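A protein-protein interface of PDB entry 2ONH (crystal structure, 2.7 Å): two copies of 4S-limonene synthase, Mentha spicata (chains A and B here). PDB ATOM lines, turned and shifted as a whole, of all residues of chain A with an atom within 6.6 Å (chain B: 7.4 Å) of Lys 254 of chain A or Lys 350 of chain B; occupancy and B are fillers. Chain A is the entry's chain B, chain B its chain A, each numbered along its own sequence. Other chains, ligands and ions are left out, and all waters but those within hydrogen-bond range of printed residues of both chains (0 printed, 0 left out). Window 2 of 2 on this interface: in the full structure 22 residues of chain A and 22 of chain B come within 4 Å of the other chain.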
ATOM      1  N   ARG A 247      -1.404   5.175   4.816  1.00  0.00           N
ATOM      2  CA  ARG A 247      -0.604   4.538   3.818  1.00  0.00           C
ATOM      3  C   ARG A 247       0.598   3.876   4.464  1.00  0.00           C
ATOM      4  O   ARG A 247       0.894   2.701   4.246  1.00  0.00           O
ATOM      5  CB  ARG A 247      -0.129   5.569   2.798  1.00  0.00           C
ATOM      6  CG  ARG A 247      -1.092   5.557   1.629  1.00  0.00           C
ATOM      7  CD  ARG A 247      -0.370   6.006   0.369  1.00  0.00           C
ATOM      8  NE  ARG A 247       0.614   5.021  -0.081  1.00  0.00           N
ATOM      9  CZ  ARG A 247       1.628   5.289  -0.932  1.00  0.00           C
ATOM     10  NH1 ARG A 247       1.786   6.520  -1.420  1.00  0.00           N
ATOM     11  NH2 ARG A 247       2.478   4.324  -1.277  1.00  0.00           N
ATOM     12  N   ASN A 248       1.282   4.660   5.273  1.00  0.00           N
ATOM     13  CA  ASN A 248       2.472   4.233   5.979  1.00  0.00           C
ATOM     14  C   ASN A 248       2.297   2.980   6.855  1.00  0.00           C
ATOM     15  O   ASN A 248       3.233   2.202   6.967  1.00  0.00           O
ATOM     16  CB  ASN A 248       2.994   5.406   6.812  1.00  0.00           C
ATOM     17  CG  ASN A 248       3.756   4.969   8.028  1.00  0.00           C
ATOM     18  OD1 ASN A 248       4.978   4.938   7.945  1.00  0.00           O
ATOM     19  ND2 ASN A 248       3.102   4.642   9.144  1.00  0.00           N
ATOM     20  N   THR A 249       1.107   2.783   7.470  1.00  0.00           N
ATOM     21  CA  THR A 249       0.876   1.613   8.315  1.00  0.00           C
ATOM     22  C   THR A 249       0.942   0.360   7.468  1.00  0.00           C
ATOM     23  O   THR A 249       1.326  -0.683   7.935  1.00  0.00           O
ATOM     24  CB  THR A 249      -0.510   1.660   9.009  1.00  0.00           C
ATOM     25  OG1 THR A 249      -1.540   1.377   8.056  1.00  0.00           O
ATOM     26  CG2 THR A 249      -0.760   3.024   9.617  1.00  0.00           C
ATOM     27  N   GLY A 250       0.557   0.494   6.215  1.00  0.00           N
ATOM     28  CA  GLY A 250       0.540  -0.588   5.236  1.00  0.00           C
ATOM     29  C   GLY A 250      -0.468  -1.674   5.559  1.00  0.00           C
ATOM     30  O   GLY A 250      -0.297  -2.789   5.119  1.00  0.00           O
ATOM     31  N   PHE A 251      -1.499  -1.360   6.317  1.00  0.00           N
ATOM     32  CA  PHE A 251      -2.489  -2.350   6.662  1.00  0.00           C
ATOM     33  C   PHE A 251      -3.149  -2.853   5.413  1.00  0.00           C
ATOM     34  O   PHE A 251      -3.531  -3.984   5.304  1.00  0.00           O
ATOM     35  CB  PHE A 251      -3.582  -1.753   7.530  1.00  0.00           C
ATOM     36  CG  PHE A 251      -3.162  -1.571   8.921  1.00  0.00           C
ATOM     37  CD1 PHE A 251      -2.046  -2.193   9.416  1.00  0.00           C
ATOM     38  CD2 PHE A 251      -3.969  -0.732   9.656  1.00  0.00           C
ATOM     39  CE1 PHE A 251      -1.717  -1.957  10.726  1.00  0.00           C
ATOM     40  CE2 PHE A 251      -3.637  -0.499  10.967  1.00  0.00           C
ATOM     41  CZ  PHE A 251      -2.512  -1.114  11.490  1.00  0.00           C
ATOM     42  N   VAL A 252      -3.298  -1.972   4.498  1.00  0.00           N
ATOM     43  CA  VAL A 252      -3.930  -2.263   3.234  1.00  0.00           C
ATOM     44  C   VAL A 252      -3.377  -3.527   2.578  1.00  0.00           C
ATOM     45  O   VAL A 252      -4.106  -4.310   1.981  1.00  0.00           O
ATOM     46  CB  VAL A 252      -3.762  -1.063   2.267  1.00  0.00           C
ATOM     47  CG1 VAL A 252      -5.093  -0.545   1.763  1.00  0.00           C
ATOM     48  CG2 VAL A 252      -3.121   0.095   3.052  1.00  0.00           C
ATOM     49  N   GLU A 253      -2.080  -3.715   2.704  1.00  0.00           N
ATOM     50  CA  GLU A 253      -1.412  -4.860   2.134  1.00  0.00           C
ATOM     51  C   GLU A 253      -1.202  -5.961   3.177  1.00  0.00           C
ATOM     52  O   GLU A 253      -1.263  -7.143   2.848  1.00  0.00           O
ATOM     53  CB  GLU A 253      -0.055  -4.432   1.548  1.00  0.00           C
ATOM     54  CG  GLU A 253       0.567  -5.312   0.449  1.00  0.00           C
ATOM     55  CD  GLU A 253       2.071  -5.758   0.499  1.00  0.00           C
ATOM     56  OE1 GLU A 253       2.344  -6.968   0.377  1.00  0.00           O
ATOM     57  OE2 GLU A 253       2.943  -4.890   0.652  1.00  0.00           O
ATOM     58  N   LYS A 254      -0.968  -5.562   4.437  1.00  0.00           N
ATOM     59  CA  LYS A 254      -0.724  -6.502   5.515  1.00  0.00           C
ATOM     60  C   LYS A 254      -1.979  -6.969   6.259  1.00  0.00           C
ATOM     61  O   LYS A 254      -2.064  -8.138   6.648  1.00  0.00           O
ATOM     62  CB  LYS A 254       0.272  -5.891   6.495  1.00  0.00           C
ATOM     63  CG  LYS A 254       1.380  -5.272   5.659  1.00  0.00           C
ATOM     64  CD  LYS A 254       2.689  -5.952   6.007  1.00  0.00           C
ATOM     65  CE  LYS A 254       3.684  -5.955   4.850  1.00  0.00           C
ATOM     66  NZ  LYS A 254       4.816  -6.924   5.049  1.00  0.00           N
ATOM     67  N   LEU A 255      -2.936  -6.065   6.467  1.00  0.00           N
ATOM     68  CA  LEU A 255      -4.201  -6.397   7.142  1.00  0.00           C
ATOM     69  C   LEU A 255      -5.327  -6.122   6.154  1.00  0.00           C
ATOM     70  O   LEU A 255      -6.199  -5.267   6.332  1.00  0.00           O
ATOM     71  CB  LEU A 255      -4.387  -5.533   8.380  1.00  0.00           C
ATOM     72  CG  LEU A 255      -4.128  -6.255   9.692  1.00  0.00           C
ATOM     73  CD1 LEU A 255      -2.799  -6.972   9.639  1.00  0.00           C
ATOM     74  CD2 LEU A 255      -4.130  -5.247  10.808  1.00  0.00           C
ATOM     75  N   PRO A 256      -5.333  -6.870   5.045  1.00  0.00           N
ATOM     76  CA  PRO A 256      -6.257  -6.836   3.931  1.00  0.00           C
ATOM     77  C   PRO A 256      -7.649  -7.394   4.199  1.00  0.00           C
ATOM     78  O   PRO A 256      -8.519  -7.257   3.341  1.00  0.00           O
ATOM     79  CB  PRO A 256      -5.531  -7.620   2.845  1.00  0.00           C
ATOM     80  CG  PRO A 256      -4.858  -8.735   3.631  1.00  0.00           C
ATOM     81  CD  PRO A 256      -4.647  -8.167   5.025  1.00  0.00           C
ATOM     82  N   PHE A 257      -7.854  -8.030   5.351  1.00  0.00           N
ATOM     83  CA  PHE A 257      -9.177  -8.568   5.701  1.00  0.00           C
ATOM     84  C   PHE A 257      -9.959  -7.388   6.283  1.00  0.00           C
ATOM     85  O   PHE A 257     -11.183  -7.443   6.462  1.00  0.00           O
ATOM     86  CB  PHE A 257      -9.041  -9.658   6.762  1.00  0.00           C
ATOM     87  CG  PHE A 257      -8.327  -9.172   7.958  1.00  0.00           C
ATOM     88  CD1 PHE A 257      -9.042  -8.608   8.989  1.00  0.00           C
ATOM     89  CD2 PHE A 257      -6.944  -9.237   7.939  1.00  0.00           C
ATOM     90  CE1 PHE A 257      -8.318  -8.081  10.034  1.00  0.00           C
ATOM     91  CE2 PHE A 257      -6.223  -8.710   8.985  1.00  0.00           C
ATOM     92  CZ  PHE A 257      -6.922  -8.132  10.026  1.00  0.00           C
ATOM     93  N   TYR A 329      -0.200 -10.697  12.079  1.00  0.00           N
ATOM     94  CA  TYR A 329      -1.025  -9.561  11.787  1.00  0.00           C
ATOM     95  C   TYR A 329      -1.413  -8.776  13.026  1.00  0.00           C
ATOM     96  O   TYR A 329      -1.669  -7.588  12.937  1.00  0.00           O
ATOM     97  CB  TYR A 329      -2.269  -9.986  11.008  1.00  0.00           C
ATOM     98  CG  TYR A 329      -3.257 -10.795  11.845  1.00  0.00           C
ATOM     99  CD1 TYR A 329      -3.240 -12.185  11.861  1.00  0.00           C
ATOM    100  CD2 TYR A 329      -4.247 -10.125  12.536  1.00  0.00           C
ATOM    101  CE1 TYR A 329      -4.218 -12.901  12.560  1.00  0.00           C
ATOM    102  CE2 TYR A 329      -5.226 -10.834  13.238  1.00  0.00           C
ATOM    103  CZ  TYR A 329      -5.210 -12.209  13.245  1.00  0.00           C
ATOM    104  OH  TYR A 329      -6.155 -12.823  13.910  1.00  0.00           O
ATOM    105  N   LEU A 332       1.614  -6.426  14.106  1.00  0.00           N
ATOM    106  CA  LEU A 332       1.635  -5.192  13.414  1.00  0.00           C
ATOM    107  C   LEU A 332       0.547  -4.300  13.963  1.00  0.00           C
ATOM    108  O   LEU A 332       0.853  -3.192  14.362  1.00  0.00           O
ATOM    109  CB  LEU A 332       1.439  -5.397  11.909  1.00  0.00           C
ATOM    110  CG  LEU A 332       2.102  -4.334  11.018  1.00  0.00           C
ATOM    111  CD1 LEU A 332       3.607  -4.489  11.033  1.00  0.00           C
ATOM    112  CD2 LEU A 332       1.720  -4.531   9.571  1.00  0.00           C
ATOM    113  N   ASP B 343       8.810   3.768  16.343  1.00  0.00           N
ATOM    114  CA  ASP B 343       8.441   4.004  14.928  1.00  0.00           C
ATOM    115  C   ASP B 343       9.410   3.302  13.997  1.00  0.00           C
ATOM    116  O   ASP B 343       9.003   2.778  12.952  1.00  0.00           O
ATOM    117  CB  ASP B 343       8.447   5.485  14.551  1.00  0.00           C
ATOM    118  CG  ASP B 343       8.676   5.697  12.998  1.00  0.00           C
ATOM    119  OD1 ASP B 343       7.955   5.063  12.197  1.00  0.00           O
ATOM    120  OD2 ASP B 343       9.573   6.480  12.609  1.00  0.00           O
ATOM    121  N   THR B 344      10.703   3.323  14.370  1.00  0.00           N
ATOM    122  CA  THR B 344      11.699   2.695  13.602  1.00  0.00           C
ATOM    123  C   THR B 344      11.539   1.171  13.637  1.00  0.00           C
ATOM    124  O   THR B 344      11.567   0.538  12.580  1.00  0.00           O
ATOM    125  CB  THR B 344      12.994   3.095  14.079  1.00  0.00           C
ATOM    126  OG1 THR B 344      13.217   4.438  13.643  1.00  0.00           O
ATOM    127  CG2 THR B 344      14.097   2.202  13.537  1.00  0.00           C
ATOM    128  N   SER B 345      11.345   0.575  14.813  1.00  0.00           N
ATOM    129  CA  SER B 345      11.172  -0.860  14.869  1.00  0.00           C
ATOM    130  C   SER B 345       9.968  -1.283  14.046  1.00  0.00           C
ATOM    131  O   SER B 345       9.916  -2.427  13.590  1.00  0.00           O
ATOM    132  CB  SER B 345      10.995  -1.317  16.301  1.00  0.00           C
ATOM    133  OG  SER B 345      11.905  -0.387  16.827  1.00  0.00           O
ATOM    134  N   TYR B 346       8.996  -0.361  13.857  1.00  0.00           N
ATOM    135  CA  TYR B 346       7.787  -0.668  13.052  1.00  0.00           C
ATOM    136  C   TYR B 346       8.053  -0.802  11.549  1.00  0.00           C
ATOM    137  O   TYR B 346       7.539  -1.709  10.924  1.00  0.00           O
ATOM    138  CB  TYR B 346       6.714   0.408  13.255  1.00  0.00           C
ATOM    139  CG  TYR B 346       5.410   0.071  12.547  1.00  0.00           C
ATOM    140  CD1 TYR B 346       4.470  -0.739  13.178  1.00  0.00           C
ATOM    141  CD2 TYR B 346       5.165   0.520  11.276  1.00  0.00           C
ATOM    142  CE1 TYR B 346       3.283  -1.117  12.537  1.00  0.00           C
ATOM    143  CE2 TYR B 346       3.983   0.152  10.630  1.00  0.00           C
ATOM    144  CZ  TYR B 346       3.059  -0.662  11.253  1.00  0.00           C
ATOM    145  OH  TYR B 346       1.998  -1.048  10.598  1.00  0.00           O
ATOM    146  N   ASP B 347       8.827   0.131  10.966  1.00  0.00           N
ATOM    147  CA  ASP B 347       9.131   0.083   9.524  1.00  0.00           C
ATOM    148  C   ASP B 347       9.890  -1.193   9.280  1.00  0.00           C
ATOM    149  O   ASP B 347       9.569  -1.975   8.402  1.00  0.00           O
ATOM    150  CB  ASP B 347      10.022   1.247   9.112  1.00  0.00           C
ATOM    151  CG  ASP B 347       9.328   2.590   9.196  1.00  0.00           C
ATOM    152  OD1 ASP B 347       8.151   2.636   9.529  1.00  0.00           O
ATOM    153  OD2 ASP B 347       9.994   3.597   8.919  1.00  0.00           O
ATOM    154  N   VAL B 348      10.918  -1.385  10.075  1.00  0.00           N
ATOM    155  CA  VAL B 348      11.723  -2.547   9.973  1.00  0.00           C
ATOM    156  C   VAL B 348      10.855  -3.783  10.114  1.00  0.00           C
ATOM    157  O   VAL B 348      11.067  -4.736   9.415  1.00  0.00           O
ATOM    158  CB  VAL B 348      12.784  -2.571  11.039  1.00  0.00           C
ATOM    159  CG1 VAL B 348      13.129  -3.986  11.433  1.00  0.00           C
ATOM    160  CG2 VAL B 348      14.015  -1.907  10.463  1.00  0.00           C
ATOM    161  N   MET B 349       9.894  -3.762  11.014  1.00  0.00           N
ATOM    162  CA  MET B 349       9.026  -4.917  11.176  1.00  0.00           C
ATOM    163  C   MET B 349       8.088  -4.972   9.978  1.00  0.00           C
ATOM    164  O   MET B 349       7.816  -6.004   9.398  1.00  0.00           O
ATOM    165  CB  MET B 349       8.211  -4.809  12.470  1.00  0.00           C
ATOM    166  CG  MET B 349       6.722  -5.194  12.439  1.00  0.00           C
ATOM    167  SD  MET B 349       6.157  -5.758  14.078  1.00  0.00           S
ATOM    168  CE  MET B 349       5.892  -7.434  13.601  1.00  0.00           C
ATOM    169  N   LYS B 350       7.605  -3.837   9.615  1.00  0.00           N
ATOM    170  CA  LYS B 350       6.730  -3.743   8.529  1.00  0.00           C
ATOM    171  C   LYS B 350       7.367  -4.288   7.263  1.00  0.00           C
ATOM    172  O   LYS B 350       6.750  -5.058   6.565  1.00  0.00           O
ATOM    173  CB  LYS B 350       6.325  -2.298   8.318  1.00  0.00           C
ATOM    174  CG  LYS B 350       5.439  -2.381   7.110  1.00  0.00           C
ATOM    175  CD  LYS B 350       4.817  -1.002   7.046  1.00  0.00           C
ATOM    176  CE  LYS B 350       5.634   0.005   6.228  1.00  0.00           C
ATOM    177  NZ  LYS B 350       6.366   1.011   7.074  1.00  0.00           N
ATOM    178  N   GLU B 351       8.601  -3.896   6.986  1.00  0.00           N
ATOM    179  CA  GLU B 351       9.264  -4.346   5.782  1.00  0.00           C
ATOM    180  C   GLU B 351      10.119  -5.606   5.884  1.00  0.00           C
ATOM    181  O   GLU B 351      10.017  -6.423   4.984  1.00  0.00           O
ATOM    182  CB  GLU B 351      10.110  -3.218   5.194  1.00  0.00           C
ATOM    183  CG  GLU B 351      11.264  -2.822   6.076  1.00  0.00           C
ATOM    184  CD  GLU B 351      11.414  -1.318   6.228  1.00  0.00           C
ATOM    185  OE1 GLU B 351      10.414  -0.609   6.063  1.00  0.00           O
ATOM    186  OE2 GLU B 351      12.536  -0.864   6.511  1.00  0.00           O
ATOM    187  N   LYS B 352      10.937  -5.775   6.948  1.00  0.00           N
ATOM    188  CA  LYS B 352      11.813  -6.967   7.065  1.00  0.00           C
ATOM    189  C   LYS B 352      11.245  -8.136   7.857  1.00  0.00           C
ATOM    190  O   LYS B 352      11.828  -9.210   7.831  1.00  0.00           O
ATOM    191  CB  LYS B 352      13.163  -6.569   7.668  1.00  0.00           C
ATOM    192  CG  LYS B 352      14.323  -6.296   6.726  1.00  0.00           C
ATOM    193  CD  LYS B 352      14.427  -4.812   6.453  1.00  0.00           C
ATOM    194  CE  LYS B 352      15.830  -4.429   6.012  1.00  0.00           C
ATOM    195  NZ  LYS B 352      16.068  -2.952   6.096  1.00  0.00           N
ATOM    196  N   GLY B 353      10.136  -7.927   8.562  1.00  0.00           N
ATOM    197  CA  GLY B 353       9.454  -8.950   9.363  1.00  0.00           C
ATOM    198  C   GLY B 353       9.905  -9.246  10.792  1.00  0.00           C
ATOM    199  O   GLY B 353       9.492 -10.264  11.360  1.00  0.00           O
ATOM    200  N   VAL B 354      10.723  -8.323  11.384  1.00  0.00           N
ATOM    201  CA  VAL B 354      11.270  -8.481  12.744  1.00  0.00           C
ATOM    202  C   VAL B 354      10.983  -7.394  13.802  1.00  0.00           C
ATOM    203  O   VAL B 354      10.903  -6.166  13.547  1.00  0.00           O
ATOM    204  CB  VAL B 354      12.764  -8.630  12.665  1.00  0.00           C
ATOM    205  CG1 VAL B 354      13.015 -10.044  12.221  1.00  0.00           C
ATOM    206  CG2 VAL B 354      13.395  -7.705  11.625  1.00  0.00           C
ATOM    207  N   ARG B 409      18.700  -1.343   8.775  1.00  0.00           N
ATOM    208  CA  ARG B 409      18.176  -0.679   7.613  1.00  0.00           C
ATOM    209  C   ARG B 409      18.928  -0.974   6.329  1.00  0.00           C
ATOM    210  O   ARG B 409      18.348  -1.056   5.241  1.00  0.00           O
ATOM    211  CB  ARG B 409      18.164   0.836   7.846  1.00  0.00           C
ATOM    212  CG  ARG B 409      17.169   1.356   8.872  1.00  0.00           C
ATOM    213  CD  ARG B 409      16.010   0.385   9.043  1.00  0.00           C
ATOM    214  NE  ARG B 409      14.801   0.771   8.314  1.00  0.00           N
ATOM    215  CZ  ARG B 409      14.243   1.989   8.349  1.00  0.00           C
ATOM    216  NH1 ARG B 409      14.782   2.959   9.073  1.00  0.00           N
ATOM    217  NH2 ARG B 409      13.130   2.227   7.675  1.00  0.00           N
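The backbone carbonyl oxygen (O) of Lys 350 of chain B sits at hydrogen-bond distance from the side-chain amino group (NZ) of Lys 254 of chain A (3.1 Å). OH of Tyr 346 of chain B is in hydrogen-bond range of O of Thr 249 of chain A (2.8 Å). The backbone carbonyl oxygen (O) of Asn 248 of chain A lies close to the side-chain amino group (NZ) of Lys 350 of chain B (3.4 Å).
The side-chain amino group of Lys 350 of chain B is in salt-bridge range of the side-chain carboxylate of Asp 347 of chain B (3.4 Å). OG1 of Thr 249 of chain A lies close to N of Phe 251 of chain A (3.2 Å).
Among the printed residues, pairs that only touch across the chains: Thr 249 of chain A with Lys 350 of chain B (3.6 Å), Phe 251 of chain A with Tyr 346 of chain B (3.8 Å), Leu 332 of chain A with Tyr 346 of chain B (3.3 Å) and Leu 332 of chain A with Met 349 of chain B (3.5 Å).
Printed residues of chain B within 4 Å of Thr 249 of chain A: Tyr 346 (2.8 Å) and Lys 350 (3.6 Å). Printed residues of chain B within 4 Å of Lys 254 of chain A: Lys 350 (3.1 Å). Of the printed residues of chain B, Leu 332 of chain A touches Tyr 346 and Met 349. Of the printed residues of chain A, Tyr 346 of chain B touches Thr 249 (2.8 Å), Phe 251 (3.8 Å) and Leu 332 (3.3 Å). Lys 350 of chain B touches three residues of chain A. Gly 353 of chain B touches none of the printed residues of chain A. The nearest residue of chain B that does not touch Lys 254 of chain A is Glu 351 of chain B (5.2 Å). The nearest residue of chain A that does not touch Lys 350 of chain B is Leu 332 of chain A (4.1 Å).
Hydrophobic or aromatic side chains of chain B within 4 Å of the printed part of chain A: Tyr 346 and Met 349. Hydrophobic or aromatic side chains of chain A that line the printed part of chain B: Phe 251 and Leu 332. Among the printed residues, no Asp or Glu carboxylate lies within 4 Å of a Lys or Arg side-chain nitrogen of the other chain.
No position is printed for both chains. Of the 7 pairs that touch across the chains among the printed residues, none has its exchanged pair printed and touching as well.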
